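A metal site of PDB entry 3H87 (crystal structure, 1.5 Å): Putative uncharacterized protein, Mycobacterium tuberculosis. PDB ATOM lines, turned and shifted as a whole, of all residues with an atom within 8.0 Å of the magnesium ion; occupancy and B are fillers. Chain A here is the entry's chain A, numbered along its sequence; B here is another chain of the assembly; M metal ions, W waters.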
ATOM      1  N   ASP A  24     -10.896  -0.601 -19.677  1.00  0.00           N
ATOM      2  CA  ASP A  24     -10.912  -0.586 -21.135  1.00  0.00           C
ATOM      3  C   ASP A  24     -10.859  -1.993 -21.712  1.00  0.00           C
ATOM      4  O   ASP A  24     -10.342  -2.912 -21.063  1.00  0.00           O
ATOM      5  CB  ASP A  24      -9.697   0.222 -21.651  1.00  0.00           C
ATOM      6  CG  ASP A  24      -9.714   0.386 -23.131  1.00  0.00           C
ATOM      7  OD1 ASP A  24     -10.682   1.030 -23.594  1.00  0.00           O
ATOM      8  OD2 ASP A  24      -8.769  -0.084 -23.820  1.00  0.00           O
ATOM      9  N   LYS A  25     -11.276  -2.151 -22.982  1.00  0.00           N
ATOM     10  CA  LYS A  25     -11.134  -3.451 -23.652  1.00  0.00           C
ATOM     11  C   LYS A  25      -9.725  -4.036 -23.611  1.00  0.00           C
ATOM     12  O   LYS A  25      -9.535  -5.261 -23.516  1.00  0.00           O
ATOM     13  CB  LYS A  25     -11.627  -3.377 -25.129  1.00  0.00           C
ATOM     14  CG  LYS A  25     -10.831  -2.394 -26.054  1.00  0.00           C
ATOM     15  CD  LYS A  25     -11.259  -2.454 -27.549  1.00  0.00           C
ATOM     16  CE  LYS A  25     -10.654  -1.387 -28.419  1.00  0.00           C
ATOM     17  NZ  LYS A  25     -11.239   0.003 -28.155  1.00  0.00           N
ATOM     18  N   SER A  26      -8.724  -3.167 -23.692  1.00  0.00           N
ATOM     19  CA  SER A  26      -7.329  -3.582 -23.737  1.00  0.00           C
ATOM     20  C   SER A  26      -6.854  -4.271 -22.450  1.00  0.00           C
ATOM     21  O   SER A  26      -5.989  -5.184 -22.495  1.00  0.00           O
ATOM     22  CB  SER A  26      -6.409  -2.379 -24.050  1.00  0.00           C
ATOM     23  OG  SER A  26      -6.520  -1.366 -23.059  1.00  0.00           O
ATOM     24  N   ARG A 108      -5.473  11.005 -34.639  1.00  0.00           N
ATOM     25  CA  ARG A 108      -5.794   9.720 -35.261  1.00  0.00           C
ATOM     26  C   ARG A 108      -5.097   8.582 -34.548  1.00  0.00           C
ATOM     27  O   ARG A 108      -5.158   7.440 -34.994  1.00  0.00           O
ATOM     28  CB  ARG A 108      -5.513   9.763 -36.736  1.00  0.00           C
ATOM     29  CG  ARG A 108      -6.400  10.822 -37.356  1.00  0.00           C
ATOM     30  CD  ARG A 108      -6.640  10.638 -38.765  1.00  0.00           C
ATOM     31  NE  ARG A 108      -7.376  11.789 -39.270  1.00  0.00           N
ATOM     32  CZ  ARG A 108      -7.270  12.225 -40.518  1.00  0.00           C
ATOM     33  NH1 ARG A 108      -6.444  11.616 -41.393  1.00  0.00           N
ATOM     34  NH2 ARG A 108      -7.982  13.261 -40.912  1.00  0.00           N
ATOM     35  N   GLY A 109      -4.491   8.888 -33.402  1.00  0.00           N
ATOM     36  CA  GLY A 109      -3.948   7.912 -32.475  1.00  0.00           C
ATOM     37  C   GLY A 109      -5.118   7.344 -31.672  1.00  0.00           C
ATOM     38  O   GLY A 109      -5.622   6.269 -31.978  1.00  0.00           O
ATOM     39  N   PRO A 110      -5.554   8.045 -30.616  1.00  0.00           N
ATOM     40  CA  PRO A 110      -6.709   7.607 -29.855  1.00  0.00           C
ATOM     41  C   PRO A 110      -8.000   7.492 -30.669  1.00  0.00           C
ATOM     42  O   PRO A 110      -8.379   8.417 -31.383  1.00  0.00           O
ATOM     43  CB  PRO A 110      -6.841   8.670 -28.775  1.00  0.00           C
ATOM     44  CG  PRO A 110      -5.465   9.288 -28.658  1.00  0.00           C
ATOM     45  CD  PRO A 110      -4.986   9.281 -30.060  1.00  0.00           C
ATOM     46  N   SER A 111      -8.654   6.364 -30.538  1.00  0.00           N
ATOM     47  CA  SER A 111      -9.921   6.113 -31.219  1.00  0.00           C
ATOM     48  C   SER A 111     -11.107   6.823 -30.518  1.00  0.00           C
ATOM     49  O   SER A 111     -10.967   7.355 -29.411  1.00  0.00           O
ATOM     50  CB  SER A 111     -10.150   4.634 -31.251  1.00  0.00           C
ATOM     51  OG  SER A 111     -10.363   4.162 -29.926  1.00  0.00           O
ATOM     52  N   ILE A 112     -12.268   6.793 -31.182  1.00  0.00           N
ATOM     53  CA  ILE A 112     -13.468   7.342 -30.580  1.00  0.00           C
ATOM     54  C   ILE A 112     -13.801   6.617 -29.261  1.00  0.00           C
ATOM     55  O   ILE A 112     -14.075   7.253 -28.243  1.00  0.00           O
ATOM     56  CB  ILE A 112     -14.622   7.471 -31.633  1.00  0.00           C
ATOM     57  CG1 ILE A 112     -14.222   8.447 -32.726  1.00  0.00           C
ATOM     58  CG2 ILE A 112     -15.926   7.898 -30.926  1.00  0.00           C
ATOM     59  CD1 ILE A 112     -15.205   8.541 -33.898  1.00  0.00           C
ATOM     60  N   PRO A 113     -13.799   5.254 -29.226  1.00  0.00           N
ATOM     61  CA  PRO A 113     -13.992   4.597 -27.941  1.00  0.00           C
ATOM     62  C   PRO A 113     -12.974   5.064 -26.867  1.00  0.00           C
ATOM     63  O   PRO A 113     -13.356   5.269 -25.721  1.00  0.00           O
ATOM     64  CB  PRO A 113     -13.894   3.085 -28.273  1.00  0.00           C
ATOM     65  CG  PRO A 113     -14.344   3.025 -29.739  1.00  0.00           C
ATOM     66  CD  PRO A 113     -13.848   4.300 -30.366  1.00  0.00           C
ATOM     67  N   ASP A 114     -11.686   5.226 -27.216  1.00  0.00           N
ATOM     68  CA  ASP A 114     -10.689   5.628 -26.220  1.00  0.00           C
ATOM     69  C   ASP A 114     -11.109   6.978 -25.622  1.00  0.00           C
ATOM     70  O   ASP A 114     -11.047   7.194 -24.388  1.00  0.00           O
ATOM     71  CB  ASP A 114      -9.282   5.753 -26.814  1.00  0.00           C
ATOM     72  CG  ASP A 114      -8.671   4.461 -27.330  1.00  0.00           C
ATOM     73  OD1 ASP A 114      -9.166   3.372 -26.997  1.00  0.00           O
ATOM     74  OD2 ASP A 114      -7.618   4.585 -28.073  1.00  0.00           O
ATOM     75  N   LEU A 115     -11.523   7.910 -26.509  1.00  0.00           N
ATOM     76  CA  LEU A 115     -11.958   9.241 -26.026  1.00  0.00           C
ATOM     77  C   LEU A 115     -13.185   9.172 -25.104  1.00  0.00           C
ATOM     78  O   LEU A 115     -13.284   9.882 -24.114  1.00  0.00           O
ATOM     79  CB  LEU A 115     -12.220  10.188 -27.180  1.00  0.00           C
ATOM     80  CG  LEU A 115     -11.003  10.572 -27.980  1.00  0.00           C
ATOM     81  CD1 LEU A 115     -11.438  11.050 -29.401  1.00  0.00           C
ATOM     82  CD2 LEU A 115     -10.228  11.665 -27.245  1.00  0.00           C
ATOM     83  N   VAL A 131      -4.360  -1.244 -21.211  1.00  0.00           N
ATOM     84  CA  VAL A 131      -3.046  -1.545 -21.812  1.00  0.00           C
ATOM     85  C   VAL A 131      -3.010  -0.898 -23.215  1.00  0.00           C
ATOM     86  O   VAL A 131      -3.080  -1.583 -24.248  1.00  0.00           O
ATOM     87  CB  VAL A 131      -2.759  -3.075 -21.900  1.00  0.00           C
ATOM     88  CG1 VAL A 131      -1.297  -3.324 -22.397  1.00  0.00           C
ATOM     89  CG2 VAL A 131      -3.017  -3.770 -20.553  1.00  0.00           C
ATOM     90  N   ASP A 132      -2.990   0.437 -23.249  1.00  0.00           N
ATOM     91  CA  ASP A 132      -3.089   1.211 -24.502  1.00  0.00           C
ATOM     92  C   ASP A 132      -2.479   2.602 -24.297  1.00  0.00           C
ATOM     93  O   ASP A 132      -3.051   3.463 -23.585  1.00  0.00           O
ATOM     94  CB  ASP A 132      -4.556   1.335 -25.000  1.00  0.00           C
ATOM     95  CG  ASP A 132      -4.690   2.042 -26.330  1.00  0.00           C
ATOM     96  OD1 ASP A 132      -3.704   2.631 -26.847  1.00  0.00           O
ATOM     97  OD2 ASP A 132      -5.834   1.993 -26.860  1.00  0.00           O
ATOM     98  N   LYS A 133      -1.331   2.825 -24.918  1.00  0.00           N
ATOM     99  CA  LYS A 133      -0.636   4.102 -24.739  1.00  0.00           C
ATOM    100  C   LYS A 133      -1.456   5.311 -25.160  1.00  0.00           C
ATOM    101  O   LYS A 133      -1.130   6.458 -24.783  1.00  0.00           O
ATOM    102  CB  LYS A 133       0.720   4.114 -25.456  1.00  0.00           C
ATOM    103  CG  LYS A 133       0.629   4.007 -26.959  1.00  0.00           C
ATOM    104  CD  LYS A 133       2.032   4.093 -27.563  1.00  0.00           C
ATOM    105  CE  LYS A 133       1.988   3.774 -29.036  1.00  0.00           C
ATOM    106  NZ  LYS A 133       1.043   4.662 -29.750  1.00  0.00           N
ATOM    107  N   ASP A 134      -2.504   5.145 -25.957  1.00  0.00           N
ATOM    108  CA  ASP A 134      -3.339   6.290 -26.273  1.00  0.00           C
ATOM    109  C   ASP A 134      -3.928   6.933 -25.020  1.00  0.00           C
ATOM    110  O   ASP A 134      -4.219   8.127 -25.033  1.00  0.00           O
ATOM    111  CB  ASP A 134      -4.465   5.897 -27.231  1.00  0.00           C
ATOM    112  CG  ASP A 134      -3.949   5.496 -28.610  1.00  0.00           C
ATOM    113  OD1 ASP A 134      -2.945   6.104 -29.053  1.00  0.00           O
ATOM    114  OD2 ASP A 134      -4.596   4.571 -29.241  1.00  0.00           O
ATOM    115  N   PHE A 135      -4.149   6.176 -23.942  1.00  0.00           N
ATOM    116  CA  PHE A 135      -4.659   6.802 -22.693  1.00  0.00           C
ATOM    117  C   PHE A 135      -3.614   7.696 -22.029  1.00  0.00           C
ATOM    118  O   PHE A 135      -3.977   8.690 -21.413  1.00  0.00           O
ATOM    119  CB  PHE A 135      -5.219   5.752 -21.725  1.00  0.00           C
ATOM    120  CG  PHE A 135      -6.471   5.119 -22.232  1.00  0.00           C
ATOM    121  CD1 PHE A 135      -7.642   5.826 -22.201  1.00  0.00           C
ATOM    122  CD2 PHE A 135      -6.472   3.828 -22.711  1.00  0.00           C
ATOM    123  CE1 PHE A 135      -8.816   5.280 -22.668  1.00  0.00           C
ATOM    124  CE2 PHE A 135      -7.650   3.284 -23.232  1.00  0.00           C
ATOM    125  CZ  PHE A 135      -8.802   4.000 -23.177  1.00  0.00           C
ATOM    126  N   ILE A 138      -3.987  11.035 -23.959  1.00  0.00           N
ATOM    127  CA  ILE A 138      -5.109  11.789 -23.481  1.00  0.00           C
ATOM    128  C   ILE A 138      -4.809  12.399 -22.079  1.00  0.00           C
ATOM    129  O   ILE A 138      -5.125  13.596 -21.853  1.00  0.00           O
ATOM    130  CB  ILE A 138      -6.383  10.888 -23.427  1.00  0.00           C
ATOM    131  CG1 ILE A 138      -6.869  10.542 -24.835  1.00  0.00           C
ATOM    132  CG2 ILE A 138      -7.509  11.603 -22.653  1.00  0.00           C
ATOM    133  CD1 ILE A 138      -7.910   9.382 -24.896  1.00  0.00           C
ATOM    134  N   GLN B  70     -10.602   2.617 -38.473  1.00  0.00           N
ATOM    135  CA  GLN B  70      -9.593   3.064 -37.502  1.00  0.00           C
ATOM    136  C   GLN B  70     -10.196   3.892 -36.350  1.00  0.00           C
ATOM    137  O   GLN B  70      -9.853   3.702 -35.177  1.00  0.00           O
ATOM    138  CB  GLN B  70      -8.518   3.868 -38.243  1.00  0.00           C
ATOM    139  CG  GLN B  70      -7.393   4.337 -37.364  1.00  0.00           C
ATOM    140  CD  GLN B  70      -6.345   5.146 -38.114  1.00  0.00           C
ATOM    141  OE1 GLN B  70      -6.260   5.088 -39.351  1.00  0.00           O
ATOM    142  NE2 GLN B  70      -5.529   5.890 -37.368  1.00  0.00           N
ATOM    143  N   ARG B  73     -11.654   1.459 -33.521  1.00  0.00           N
ATOM    144  CA  ARG B  73     -10.838   0.473 -32.830  1.00  0.00           C
ATOM    145  C   ARG B  73     -10.408   0.945 -31.466  1.00  0.00           C
ATOM    146  O   ARG B  73      -9.329   0.590 -31.004  1.00  0.00           O
ATOM    147  CB  ARG B  73      -9.569   0.206 -33.605  1.00  0.00           C
ATOM    148  CG  ARG B  73      -9.693  -0.451 -34.888  1.00  0.00           C
ATOM    149  CD  ARG B  73     -10.903  -1.342 -35.020  1.00  0.00           C
ATOM    150  NE  ARG B  73     -11.986  -0.633 -35.738  1.00  0.00           N
ATOM    151  CZ  ARG B  73     -12.801  -1.129 -36.689  1.00  0.00           C
ATOM    152  NH1 ARG B  73     -13.707  -0.289 -37.227  1.00  0.00           N
ATOM    153  NH2 ARG B  73     -12.731  -2.409 -37.172  1.00  0.00           N
ATOM    154  OXT ARG B  73     -11.057   1.670 -30.745  1.00  0.00           O
HETATM  155 MG    MG M   1      -6.201   2.969 -28.913  1.00  0.00          MG
HETATM  156  O   HOH W   1      -5.035   1.356 -30.038  1.00  0.00           O
HETATM  157  O   HOH W   2      -6.687   3.749 -31.070  1.00  0.00           O
HETATM  158  O   HOH W   3      -8.041   1.685 -29.011  1.00  0.00           O
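The backbone NH (N) of Asp 114 lies close to the side-chain hydroxyl (OG) of Ser 111, at 3.2 Å.
Three residues have an atom within 4 Å of the magnesium ion: Asp 114, Asp 132 and Asp 134.
The nearest printed residue that does not touch the magnesium ion is Ser 111 (4.4 Å).
The magnesium ion is bound by water W3 (2.2 Å), water W1 (2.3 Å), the side-chain carboxylate (OD2) of Asp 134 (2.3 Å), the side-chain carboxylate (OD2) of Asp 132 (2.3 Å), the side-chain carboxylate (OD2) of Asp 114 (2.3 Å) and water W2 (2.3 Å).
Water W3 bridges O of Arg 73 of chain B (2.6 Å) and OD1 of Asp 114 (2.9 Å).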
